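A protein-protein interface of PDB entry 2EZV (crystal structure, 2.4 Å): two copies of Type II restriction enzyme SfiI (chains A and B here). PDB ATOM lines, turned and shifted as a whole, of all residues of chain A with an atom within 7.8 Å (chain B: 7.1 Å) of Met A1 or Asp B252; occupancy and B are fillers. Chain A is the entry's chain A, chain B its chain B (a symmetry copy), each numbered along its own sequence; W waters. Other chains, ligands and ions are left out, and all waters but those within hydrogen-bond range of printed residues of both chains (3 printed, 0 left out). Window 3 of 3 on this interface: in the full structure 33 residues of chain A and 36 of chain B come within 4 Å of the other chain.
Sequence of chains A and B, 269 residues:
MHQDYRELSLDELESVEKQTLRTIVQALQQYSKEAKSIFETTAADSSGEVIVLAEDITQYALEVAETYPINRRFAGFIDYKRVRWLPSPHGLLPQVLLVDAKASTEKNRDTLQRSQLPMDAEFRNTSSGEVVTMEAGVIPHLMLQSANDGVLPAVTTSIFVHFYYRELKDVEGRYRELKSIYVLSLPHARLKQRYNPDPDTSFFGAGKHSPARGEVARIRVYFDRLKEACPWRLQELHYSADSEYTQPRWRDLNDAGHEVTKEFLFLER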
ATOM      1  N   MET A   1      10.374  24.364  -1.905  1.00  0.00           N
ATOM      2  CA  MET A   1       9.862  23.489  -2.992  1.00  0.00           C
ATOM      3  C   MET A   1      10.588  22.158  -3.030  1.00  0.00           C
ATOM      4  O   MET A   1      11.672  22.004  -2.451  1.00  0.00           O
ATOM      5  CB  MET A   1      10.001  24.171  -4.351  1.00  0.00           C
ATOM      6  CG  MET A   1       9.123  25.400  -4.514  1.00  0.00           C
ATOM      7  SD  MET A   1       9.293  26.126  -6.153  1.00  0.00           S
ATOM      8  CE  MET A   1       7.572  26.032  -6.757  1.00  0.00           C
ATOM      9  N   HIS A   2       9.984  21.202  -3.729  1.00  0.00           N
ATOM     10  CA  HIS A   2      10.535  19.864  -3.844  1.00  0.00           C
ATOM     11  C   HIS A   2      10.504  19.360  -5.275  1.00  0.00           C
ATOM     12  O   HIS A   2       9.775  19.877  -6.119  1.00  0.00           O
ATOM     13  CB  HIS A   2       9.732  18.885  -2.988  1.00  0.00           C
ATOM     14  CG  HIS A   2       9.572  19.306  -1.564  1.00  0.00           C
ATOM     15  ND1 HIS A   2      10.451  18.926  -0.572  1.00  0.00           N
ATOM     16  CD2 HIS A   2       8.613  20.045  -0.955  1.00  0.00           C
ATOM     17  CE1 HIS A   2      10.040  19.410   0.587  1.00  0.00           C
ATOM     18  NE2 HIS A   2       8.925  20.091   0.382  1.00  0.00           N
ATOM     19  N   GLN A   3      11.305  18.333  -5.523  1.00  0.00           N
ATOM     20  CA  GLN A   3      11.362  17.693  -6.820  1.00  0.00           C
ATOM     21  C   GLN A   3      10.987  16.219  -6.615  1.00  0.00           C
ATOM     22  O   GLN A   3      10.503  15.556  -7.531  1.00  0.00           O
ATOM     23  CB  GLN A   3      12.768  17.814  -7.404  1.00  0.00           C
ATOM     24  CG  GLN A   3      13.173  19.240  -7.741  1.00  0.00           C
ATOM     25  CD  GLN A   3      14.456  19.288  -8.543  1.00  0.00           C
ATOM     26  OE1 GLN A   3      15.525  18.913  -8.057  1.00  0.00           O
ATOM     27  NE2 GLN A   3      14.355  19.745  -9.791  1.00  0.00           N
ATOM     28  N   ASP A   4      11.223  15.725  -5.399  1.00  0.00           N
ATOM     29  CA  ASP A   4      10.913  14.348  -5.020  1.00  0.00           C
ATOM     30  C   ASP A   4       9.553  14.332  -4.291  1.00  0.00           C
ATOM     31  O   ASP A   4       9.441  14.816  -3.170  1.00  0.00           O
ATOM     32  CB  ASP A   4      12.000  13.809  -4.087  1.00  0.00           C
ATOM     33  CG  ASP A   4      11.944  12.301  -3.941  1.00  0.00           C
ATOM     34  OD1 ASP A   4      10.837  11.753  -3.787  1.00  0.00           O
ATOM     35  OD2 ASP A   4      13.008  11.659  -3.983  1.00  0.00           O
ATOM     36  N   GLU A   7       8.939  13.564  -0.611  1.00  0.00           N
ATOM     37  CA  GLU A   7       9.192  14.590   0.397  1.00  0.00           C
ATOM     38  C   GLU A   7       7.915  15.363   0.737  1.00  0.00           C
ATOM     39  O   GLU A   7       7.869  16.067   1.743  1.00  0.00           O
ATOM     40  CB  GLU A   7      10.265  15.570  -0.093  1.00  0.00           C
ATOM     41  CG  GLU A   7      11.697  15.058   0.054  1.00  0.00           C
ATOM     42  CD  GLU A   7      12.731  15.946  -0.636  1.00  0.00           C
ATOM     43  OE1 GLU A   7      12.591  17.191  -0.608  1.00  0.00           O
ATOM     44  OE2 GLU A   7      13.702  15.400  -1.195  1.00  0.00           O
ATOM     45  N   LEU A   8       6.878  15.232  -0.088  1.00  0.00           N
ATOM     46  CA  LEU A   8       5.621  15.937   0.155  1.00  0.00           C
ATOM     47  C   LEU A   8       4.762  15.254   1.209  1.00  0.00           C
ATOM     48  O   LEU A   8       4.811  14.036   1.376  1.00  0.00           O
ATOM     49  CB  LEU A   8       4.788  16.021  -1.123  1.00  0.00           C
ATOM     50  CG  LEU A   8       5.369  16.648  -2.388  1.00  0.00           C
ATOM     51  CD1 LEU A   8       4.307  16.601  -3.473  1.00  0.00           C
ATOM     52  CD2 LEU A   8       5.815  18.078  -2.118  1.00  0.00           C
ATOM     53  N   PRO A  87       3.662  21.954 -13.117  1.00  0.00           N
ATOM     54  CA  PRO A  87       3.886  23.130 -12.276  1.00  0.00           C
ATOM     55  C   PRO A  87       2.986  23.111 -11.043  1.00  0.00           C
ATOM     56  O   PRO A  87       1.782  22.855 -11.123  1.00  0.00           O
ATOM     57  CB  PRO A  87       3.623  24.307 -13.227  1.00  0.00           C
ATOM     58  CG  PRO A  87       2.795  23.728 -14.322  1.00  0.00           C
ATOM     59  CD  PRO A  87       3.364  22.343 -14.505  1.00  0.00           C
ATOM     60  N   SER A  88       3.587  23.369  -9.892  1.00  0.00           N
ATOM     61  CA  SER A  88       2.849  23.350  -8.645  1.00  0.00           C
ATOM     62  C   SER A  88       3.548  24.197  -7.600  1.00  0.00           C
ATOM     63  O   SER A  88       4.751  24.423  -7.679  1.00  0.00           O
ATOM     64  CB  SER A  88       2.733  21.899  -8.157  1.00  0.00           C
ATOM     65  OG  SER A  88       2.462  21.831  -6.772  1.00  0.00           O
ATOM     66  N   PRO A  89       2.795  24.688  -6.607  1.00  0.00           N
ATOM     67  CA  PRO A  89       3.406  25.506  -5.557  1.00  0.00           C
ATOM     68  C   PRO A  89       4.376  24.689  -4.703  1.00  0.00           C
ATOM     69  O   PRO A  89       5.255  25.248  -4.047  1.00  0.00           O
ATOM     70  CB  PRO A  89       2.198  26.008  -4.764  1.00  0.00           C
ATOM     71  CG  PRO A  89       1.204  24.923  -4.947  1.00  0.00           C
ATOM     72  CD  PRO A  89       1.339  24.597  -6.413  1.00  0.00           C
ATOM     73  N   HIS A  90       4.210  23.367  -4.712  1.00  0.00           N
ATOM     74  CA  HIS A  90       5.087  22.483  -3.943  1.00  0.00           C
ATOM     75  C   HIS A  90       6.375  22.208  -4.713  1.00  0.00           C
ATOM     76  O   HIS A  90       7.270  21.530  -4.210  1.00  0.00           O
ATOM     77  CB  HIS A  90       4.401  21.146  -3.650  1.00  0.00           C
ATOM     78  CG  HIS A  90       3.037  21.285  -3.052  1.00  0.00           C
ATOM     79  ND1 HIS A  90       2.794  22.019  -1.911  1.00  0.00           N
ATOM     80  CD2 HIS A  90       1.835  20.812  -3.458  1.00  0.00           C
ATOM     81  CE1 HIS A  90       1.501  21.998  -1.644  1.00  0.00           C
ATOM     82  NE2 HIS A  90       0.896  21.273  -2.569  1.00  0.00           N
ATOM     83  N   GLY A  91       6.445  22.728  -5.936  1.00  0.00           N
ATOM     84  CA  GLY A  91       7.613  22.531  -6.779  1.00  0.00           C
ATOM     85  C   GLY A  91       7.220  22.078  -8.179  1.00  0.00           C
ATOM     86  O   GLY A  91       6.054  21.745  -8.420  1.00  0.00           O
ATOM     87  N   LEU A  92       8.171  22.094  -9.109  1.00  0.00           N
ATOM     88  CA  LEU A  92       7.905  21.633 -10.469  1.00  0.00           C
ATOM     89  C   LEU A  92       8.062  20.127 -10.343  1.00  0.00           C
ATOM     90  O   LEU A  92       9.183  19.604 -10.311  1.00  0.00           O
ATOM     91  CB  LEU A  92       8.933  22.179 -11.458  1.00  0.00           C
ATOM     92  CG  LEU A  92       8.641  21.811 -12.915  1.00  0.00           C
ATOM     93  CD1 LEU A  92       7.372  22.520 -13.397  1.00  0.00           C
ATOM     94  CD2 LEU A  92       9.813  22.199 -13.782  1.00  0.00           C
ATOM     95  N   LEU A  93       6.938  19.428 -10.270  1.00  0.00           N
ATOM     96  CA  LEU A  93       6.971  17.994 -10.064  1.00  0.00           C
ATOM     97  C   LEU A  93       6.990  17.108 -11.295  1.00  0.00           C
ATOM     98  O   LEU A  93       6.142  17.222 -12.167  1.00  0.00           O
ATOM     99  CB  LEU A  93       5.794  17.591  -9.174  1.00  0.00           C
ATOM    100  CG  LEU A  93       5.611  18.451  -7.916  1.00  0.00           C
ATOM    101  CD1 LEU A  93       4.349  18.007  -7.163  1.00  0.00           C
ATOM    102  CD2 LEU A  93       6.839  18.335  -7.030  1.00  0.00           C
ATOM    103  N   SER B  15       1.718  32.879  -5.148  1.00  0.00           N
ATOM    104  CA  SER B  15       2.026  31.474  -5.298  1.00  0.00           C
ATOM    105  C   SER B  15       1.997  31.037  -6.759  1.00  0.00           C
ATOM    106  O   SER B  15       2.864  30.276  -7.194  1.00  0.00           O
ATOM    107  CB  SER B  15       1.036  30.640  -4.480  1.00  0.00           C
ATOM    108  OG  SER B  15       1.314  29.262  -4.605  1.00  0.00           O
ATOM    109  N   LYS B  18       4.940  32.342  -8.465  1.00  0.00           N
ATOM    110  CA  LYS B  18       6.098  31.560  -8.064  1.00  0.00           C
ATOM    111  C   LYS B  18       6.230  30.265  -8.865  1.00  0.00           C
ATOM    112  O   LYS B  18       7.319  29.940  -9.326  1.00  0.00           O
ATOM    113  CB  LYS B  18       6.023  31.232  -6.572  1.00  0.00           C
ATOM    114  CG  LYS B  18       7.326  30.722  -5.985  1.00  0.00           C
ATOM    115  CD  LYS B  18       7.126  30.393  -4.522  1.00  0.00           C
ATOM    116  CE  LYS B  18       8.422  30.031  -3.834  1.00  0.00           C
ATOM    117  NZ  LYS B  18       8.193  29.643  -2.405  1.00  0.00           N
ATOM    118  N   GLN B  19       5.133  29.526  -9.043  1.00  0.00           N
ATOM    119  CA  GLN B  19       5.234  28.282  -9.803  1.00  0.00           C
ATOM    120  C   GLN B  19       5.426  28.572 -11.290  1.00  0.00           C
ATOM    121  O   GLN B  19       6.002  27.768 -12.019  1.00  0.00           O
ATOM    122  CB  GLN B  19       4.023  27.358  -9.557  1.00  0.00           C
ATOM    123  CG  GLN B  19       2.707  27.741 -10.219  1.00  0.00           C
ATOM    124  CD  GLN B  19       1.618  26.694  -9.976  1.00  0.00           C
ATOM    125  OE1 GLN B  19       1.251  26.426  -8.838  1.00  0.00           O
ATOM    126  NE2 GLN B  19       1.101  26.106 -11.047  1.00  0.00           N
ATOM    127  N   THR B  20       4.958  29.730 -11.739  1.00  0.00           N
ATOM    128  CA  THR B  20       5.144  30.117 -13.137  1.00  0.00           C
ATOM    129  C   THR B  20       6.648  30.344 -13.312  1.00  0.00           C
ATOM    130  O   THR B  20       7.269  29.830 -14.240  1.00  0.00           O
ATOM    131  CB  THR B  20       4.403  31.419 -13.465  1.00  0.00           C
ATOM    132  OG1 THR B  20       2.993  31.186 -13.415  1.00  0.00           O
ATOM    133  CG2 THR B  20       4.785  31.933 -14.848  1.00  0.00           C
ATOM    134  N   ARG B  22       9.165  29.252 -11.374  1.00  0.00           N
ATOM    135  CA  ARG B  22       9.900  28.006 -11.181  1.00  0.00           C
ATOM    136  C   ARG B  22       9.975  27.178 -12.461  1.00  0.00           C
ATOM    137  O   ARG B  22      11.039  26.675 -12.819  1.00  0.00           O
ATOM    138  CB  ARG B  22       9.258  27.163 -10.072  1.00  0.00           C
ATOM    139  CG  ARG B  22      10.054  25.913  -9.745  1.00  0.00           C
ATOM    140  CD  ARG B  22      11.464  26.281  -9.275  1.00  0.00           C
ATOM    141  NE  ARG B  22      12.321  25.114  -9.069  1.00  0.00           N
ATOM    142  CZ  ARG B  22      12.841  24.382 -10.050  1.00  0.00           C
ATOM    143  NH1 ARG B  22      12.592  24.692 -11.318  1.00  0.00           N
ATOM    144  NH2 ARG B  22      13.624  23.342  -9.766  1.00  0.00           N
ATOM    145  N   THR B  23       8.838  27.038 -13.138  1.00  0.00           N
ATOM    146  CA  THR B  23       8.758  26.280 -14.389  1.00  0.00           C
ATOM    147  C   THR B  23       9.723  26.863 -15.421  1.00  0.00           C
ATOM    148  O   THR B  23      10.470  26.136 -16.088  1.00  0.00           O
ATOM    149  CB  THR B  23       7.326  26.335 -14.960  1.00  0.00           C
ATOM    150  OG1 THR B  23       6.406  25.849 -13.977  1.00  0.00           O
ATOM    151  CG2 THR B  23       7.207  25.492 -16.209  1.00  0.00           C
ATOM    152  N   PRO B 231      12.859  37.240  -1.875  1.00  0.00           N
ATOM    153  CA  PRO B 231      13.947  36.433  -2.429  1.00  0.00           C
ATOM    154  C   PRO B 231      13.673  35.631  -3.700  1.00  0.00           C
ATOM    155  O   PRO B 231      14.462  35.694  -4.646  1.00  0.00           O
ATOM    156  CB  PRO B 231      14.338  35.535  -1.256  1.00  0.00           C
ATOM    157  CG  PRO B 231      14.095  36.416  -0.078  1.00  0.00           C
ATOM    158  CD  PRO B 231      12.758  37.045  -0.416  1.00  0.00           C
ATOM    159  N   TRP B 232      12.573  34.877  -3.737  1.00  0.00           N
ATOM    160  CA  TRP B 232      12.300  34.054  -4.911  1.00  0.00           C
ATOM    161  C   TRP B 232      11.968  34.808  -6.181  1.00  0.00           C
ATOM    162  O   TRP B 232      12.029  34.242  -7.265  1.00  0.00           O
ATOM    163  CB  TRP B 232      11.203  33.015  -4.634  1.00  0.00           C
ATOM    164  CG  TRP B 232       9.845  33.562  -4.318  1.00  0.00           C
ATOM    165  CD1 TRP B 232       9.292  33.699  -3.084  1.00  0.00           C
ATOM    166  CD2 TRP B 232       8.853  34.008  -5.255  1.00  0.00           C
ATOM    167  NE1 TRP B 232       8.014  34.197  -3.188  1.00  0.00           N
ATOM    168  CE2 TRP B 232       7.720  34.396  -4.509  1.00  0.00           C
ATOM    169  CE3 TRP B 232       8.812  34.117  -6.650  1.00  0.00           C
ATOM    170  CZ2 TRP B 232       6.554  34.886  -5.112  1.00  0.00           C
ATOM    171  CZ3 TRP B 232       7.651  34.606  -7.252  1.00  0.00           C
ATOM    172  CH2 TRP B 232       6.540  34.985  -6.481  1.00  0.00           C
ATOM    173  N   ARG B 233      11.621  36.081  -6.063  1.00  0.00           N
ATOM    174  CA  ARG B 233      11.298  36.863  -7.248  1.00  0.00           C
ATOM    175  C   ARG B 233      12.528  37.222  -8.074  1.00  0.00           C
ATOM    176  O   ARG B 233      12.413  37.842  -9.123  1.00  0.00           O
ATOM    177  CB  ARG B 233      10.535  38.128  -6.864  1.00  0.00           C
ATOM    178  CG  ARG B 233       9.079  37.856  -6.535  1.00  0.00           C
ATOM    179  CD  ARG B 233       8.299  39.133  -6.285  1.00  0.00           C
ATOM    180  NE  ARG B 233       6.904  38.837  -5.984  1.00  0.00           N
ATOM    181  CZ  ARG B 233       5.981  38.529  -6.892  1.00  0.00           C
ATOM    182  NH1 ARG B 233       6.296  38.480  -8.175  1.00  0.00           N
ATOM    183  NH2 ARG B 233       4.741  38.255  -6.510  1.00  0.00           N
ATOM    184  N   LEU B 234      13.702  36.832  -7.598  1.00  0.00           N
ATOM    185  CA  LEU B 234      14.947  37.095  -8.309  1.00  0.00           C
ATOM    186  C   LEU B 234      15.766  35.809  -8.326  1.00  0.00           C
ATOM    187  O   LEU B 234      16.258  35.358  -7.291  1.00  0.00           O
ATOM    188  CB  LEU B 234      15.729  38.216  -7.618  1.00  0.00           C
ATOM    189  CG  LEU B 234      17.012  38.796  -8.239  1.00  0.00           C
ATOM    190  CD1 LEU B 234      18.175  37.862  -8.002  1.00  0.00           C
ATOM    191  CD2 LEU B 234      16.809  39.056  -9.721  1.00  0.00           C
ATOM    192  N   GLN B 235      15.892  35.213  -9.506  1.00  0.00           N
ATOM    193  CA  GLN B 235      16.654  33.981  -9.661  1.00  0.00           C
ATOM    194  C   GLN B 235      17.901  34.244 -10.497  1.00  0.00           C
ATOM    195  O   GLN B 235      17.954  35.191 -11.278  1.00  0.00           O
ATOM    196  CB  GLN B 235      15.803  32.909 -10.342  1.00  0.00           C
ATOM    197  CG  GLN B 235      14.544  32.527  -9.592  1.00  0.00           C
ATOM    198  CD  GLN B 235      14.826  31.979  -8.210  1.00  0.00           C
ATOM    199  OE1 GLN B 235      15.764  31.212  -8.014  1.00  0.00           O
ATOM    200  NE2 GLN B 235      13.995  32.357  -7.242  1.00  0.00           N
ATOM    201  N   TRP B 250      18.248  27.430  -7.094  1.00  0.00           N
ATOM    202  CA  TRP B 250      16.946  28.060  -6.926  1.00  0.00           C
ATOM    203  C   TRP B 250      16.905  28.757  -5.587  1.00  0.00           C
ATOM    204  O   TRP B 250      17.225  28.162  -4.560  1.00  0.00           O
ATOM    205  CB  TRP B 250      15.815  27.023  -7.021  1.00  0.00           C
ATOM    206  CG  TRP B 250      14.473  27.533  -6.550  1.00  0.00           C
ATOM    207  CD1 TRP B 250      13.901  27.318  -5.331  1.00  0.00           C
ATOM    208  CD2 TRP B 250      13.551  28.355  -7.287  1.00  0.00           C
ATOM    209  NE1 TRP B 250      12.679  27.950  -5.259  1.00  0.00           N
ATOM    210  CE2 TRP B 250      12.440  28.594  -6.442  1.00  0.00           C
ATOM    211  CE3 TRP B 250      13.556  28.911  -8.578  1.00  0.00           C
ATOM    212  CZ2 TRP B 250      11.343  29.366  -6.843  1.00  0.00           C
ATOM    213  CZ3 TRP B 250      12.467  29.679  -8.978  1.00  0.00           C
ATOM    214  CH2 TRP B 250      11.372  29.898  -8.109  1.00  0.00           C
ATOM    215  N   ARG B 251      16.529  30.034  -5.624  1.00  0.00           N
ATOM    216  CA  ARG B 251      16.426  30.876  -4.437  1.00  0.00           C
ATOM    217  C   ARG B 251      14.969  30.919  -3.980  1.00  0.00           C
ATOM    218  O   ARG B 251      14.058  31.182  -4.772  1.00  0.00           O
ATOM    219  CB  ARG B 251      16.925  32.293  -4.759  1.00  0.00           C
ATOM    220  CG  ARG B 251      16.743  33.297  -3.631  1.00  0.00           C
ATOM    221  CD  ARG B 251      17.240  34.671  -4.048  1.00  0.00           C
ATOM    222  NE  ARG B 251      18.696  34.713  -4.118  1.00  0.00           N
ATOM    223  CZ  ARG B 251      19.394  35.129  -5.172  1.00  0.00           C
ATOM    224  NH1 ARG B 251      18.776  35.549  -6.273  1.00  0.00           N
ATOM    225  NH2 ARG B 251      20.721  35.127  -5.118  1.00  0.00           N
ATOM    226  N   ASP B 252      14.760  30.678  -2.692  1.00  0.00           N
ATOM    227  CA  ASP B 252      13.418  30.654  -2.135  1.00  0.00           C
ATOM    228  C   ASP B 252      13.453  31.222  -0.721  1.00  0.00           C
ATOM    229  O   ASP B 252      14.484  31.723  -0.273  1.00  0.00           O
ATOM    230  CB  ASP B 252      12.925  29.209  -2.089  1.00  0.00           C
ATOM    231  CG  ASP B 252      11.452  29.085  -2.388  1.00  0.00           C
ATOM    232  OD1 ASP B 252      10.679  29.958  -1.934  1.00  0.00           O
ATOM    233  OD2 ASP B 252      11.073  28.105  -3.068  1.00  0.00           O
ATOM    234  N   LEU B 253      12.330  31.146  -0.017  1.00  0.00           N
ATOM    235  CA  LEU B 253      12.291  31.634   1.352  1.00  0.00           C
ATOM    236  C   LEU B 253      11.587  30.630   2.254  1.00  0.00           C
ATOM    237  O   LEU B 253      10.534  30.105   1.907  1.00  0.00           O
ATOM    238  CB  LEU B 253      11.593  32.999   1.428  1.00  0.00           C
ATOM    239  CG  LEU B 253      10.103  33.092   1.770  1.00  0.00           C
ATOM    240  CD1 LEU B 253       9.719  34.557   1.877  1.00  0.00           C
ATOM    241  CD2 LEU B 253       9.261  32.392   0.706  1.00  0.00           C
ATOM    242  N   ASN B 254      12.198  30.352   3.401  1.00  0.00           N
ATOM    243  CA  ASN B 254      11.643  29.421   4.383  1.00  0.00           C
ATOM    244  C   ASN B 254      10.228  29.793   4.789  1.00  0.00           C
ATOM    245  O   ASN B 254       9.742  30.883   4.478  1.00  0.00           O
ATOM    246  CB  ASN B 254      12.525  29.370   5.631  1.00  0.00           C
ATOM    247  CG  ASN B 254      13.764  28.518   5.434  1.00  0.00           C
ATOM    248  OD1 ASN B 254      13.768  27.589   4.627  1.00  0.00           O
ATOM    249  ND2 ASN B 254      14.819  28.831   6.175  1.00  0.00           N
ATOM    250  N   HIS B 258      13.010  33.086   6.144  1.00  0.00           N
ATOM    251  CA  HIS B 258      14.421  33.336   5.872  1.00  0.00           C
ATOM    252  C   HIS B 258      14.767  32.922   4.440  1.00  0.00           C
ATOM    253  O   HIS B 258      14.106  32.058   3.855  1.00  0.00           O
ATOM    254  CB  HIS B 258      15.288  32.571   6.865  1.00  0.00           C
ATOM    255  N   GLU B 259      15.804  33.534   3.876  1.00  0.00           N
ATOM    256  CA  GLU B 259      16.210  33.222   2.510  1.00  0.00           C
ATOM    257  C   GLU B 259      17.012  31.934   2.454  1.00  0.00           C
ATOM    258  O   GLU B 259      17.816  31.652   3.332  1.00  0.00           O
ATOM    259  CB  GLU B 259      17.034  34.364   1.921  1.00  0.00           C
ATOM    260  CG  GLU B 259      17.267  34.237   0.428  1.00  0.00           C
ATOM    261  CD  GLU B 259      18.135  35.352  -0.126  1.00  0.00           C
ATOM    262  OE1 GLU B 259      17.832  36.534   0.141  1.00  0.00           O
ATOM    263  OE2 GLU B 259      19.117  35.041  -0.837  1.00  0.00           O
ATOM    264  N   VAL B 260      16.793  31.153   1.405  1.00  0.00           N
ATOM    265  CA  VAL B 260      17.490  29.889   1.248  1.00  0.00           C
ATOM    266  C   VAL B 260      17.785  29.615  -0.218  1.00  0.00           C
ATOM    267  O   VAL B 260      17.091  30.113  -1.108  1.00  0.00           O
ATOM    268  CB  VAL B 260      16.643  28.728   1.814  1.00  0.00           C
ATOM    269  CG1 VAL B 260      17.310  27.389   1.525  1.00  0.00           C
ATOM    270  CG2 VAL B 260      16.470  28.904   3.311  1.00  0.00           C
ATOM    271  N   THR B 261      18.824  28.827  -0.460  1.00  0.00           N
ATOM    272  CA  THR B 261      19.203  28.451  -1.810  1.00  0.00           C
ATOM    273  C   THR B 261      19.429  26.959  -1.797  1.00  0.00           C
ATOM    274  O   THR B 261      19.856  26.390  -0.793  1.00  0.00           O
ATOM    275  CB  THR B 261      20.500  29.163  -2.278  1.00  0.00           C
ATOM    276  OG1 THR B 261      20.186  30.492  -2.715  1.00  0.00           O
ATOM    277  CG2 THR B 261      21.151  28.410  -3.420  1.00  0.00           C
ATOM    278  N   LYS B 262      19.128  26.329  -2.918  1.00  0.00           N
ATOM    279  CA  LYS B 262      19.293  24.903  -3.050  1.00  0.00           C
ATOM    280  C   LYS B 262      19.648  24.643  -4.496  1.00  0.00           C
ATOM    281  O   LYS B 262      19.387  25.475  -5.364  1.00  0.00           O
ATOM    282  CB  LYS B 262      17.979  24.183  -2.723  1.00  0.00           C
ATOM    283  CG  LYS B 262      16.811  24.596  -3.632  1.00  0.00           C
ATOM    284  CD  LYS B 262      15.565  23.735  -3.437  1.00  0.00           C
ATOM    285  CE  LYS B 262      15.774  22.332  -3.964  1.00  0.00           C
ATOM    286  NZ  LYS B 262      14.523  21.518  -3.936  1.00  0.00           N
HETATM  287  O   HOH W   1       5.887  27.964  -2.637  1.00  0.00           O
HETATM  288  O   HOH W   2       8.878  26.828  -1.267  1.00  0.00           O
HETATM  289  O   HOH W   3      11.770  20.717 -10.452  1.00  0.00           O
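N of His A90 lies close to OG of Ser A88, 3.1 Å away. NZ of Lys B18 is in salt-bridge range of OD1 of Asp B252. OG1 of Thr B23 is in hydrogen-bond range of O of Gln B19. NE1 of Trp B250 lies within hydrogen-bond range of OD2 of Asp B252, 2.7 Å away. N of Trp B250 lies within hydrogen-bond range of O of Lys B262, 2.8 Å away. N of Asp B252 is in hydrogen-bond range of O of Val B260.
The backbone carbonyl oxygen of Met A1 lies within hydrogen-bond range of the side-chain amino group of Lys B262 (3.3 Å). The backbone carbonyl oxygen (O) of Pro A87 lies within hydrogen-bond range of the side-chain amide nitrogen (NE2) of Gln B19 (3.3 Å). The backbone nitrogen (N) of Pro A89 lies close to the side-chain amide oxygen (OE1) of Gln B19 (3.2 Å).
SD of Met A1 touches CG of Arg B22, 3.7 Å away. CZ2 of Trp B250 touches SD of Met A1 (3.9 Å). CG of Met A1 touches OD2 of Asp B252, 3.6 Å away. NE2 of Gln A3 touches NH2 of Arg B22 (3.7 Å). Pro A87 touches Thr B23. C of Ser A88 touches OE1 of Gln B19, 3.4 Å away. Ser B15 touches Pro A89. Thr B23 touches Leu A92.
No position is printed for both chains. Of the 11 pairs that touch across the chains among the printed residues, none has its exchanged pair printed and touching as well.
Of chain B, only Arg B22, Trp B250, Asp B252 and Lys B262 come within 4 Å of Met A1. Of the printed residues of chain B, Ser A88 touches Gln B19. Printed residues of chain B within 4 Å of Pro A89: Ser B15 (3.4 Å) and Gln B19 (3.0 Å). Of the printed residues of chain A, Ser B15 touches Pro A89 (3.4 Å). Printed residues of chain A within 4 Å of Thr B23: Pro A87 (3.3 Å) and Leu A92 (3.5 Å). Pro B231 touches none of the printed residues of chain A. Of chain A, only Met A1 comes within 4 Å of Asp B252. The nearest printed residue of chain A that does not touch Trp B250 is His A2 (7.4 Å).
Water W3 lies within hydrogen-bond range of the backbone carbonyl oxygen (O) of Leu A92 (2.8 Å), the side-chain amide nitrogen (NE2) of Gln A3 (2.8 Å) and the guanidinium group (NH2) of Arg B22 (3.3 Å). Water W1 bridges the side-chain amino group (NZ) of Lys B18 (2.9 Å) and the backbone carbonyl oxygen (O) of Pro A89 (3.1 Å). Water W2 lies within hydrogen-bond range of N of Met A1, NZ of Lys B18 and OD2 of Asp B252.
Printed residues of chain A that touch a printed residue of chain B: Met A1, Gln A3, Pro A87, Ser A88, Pro A89 and Leu A92. Hydrophobic or aromatic side chains of chain A within 4 Å of the printed part of chain B: Met A1, Pro A87, Pro A89 and Leu A92. Among the printed residues, no Asp or Glu carboxylate lies within 4 Å of a Lys or Arg side-chain nitrogen of the other chain.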
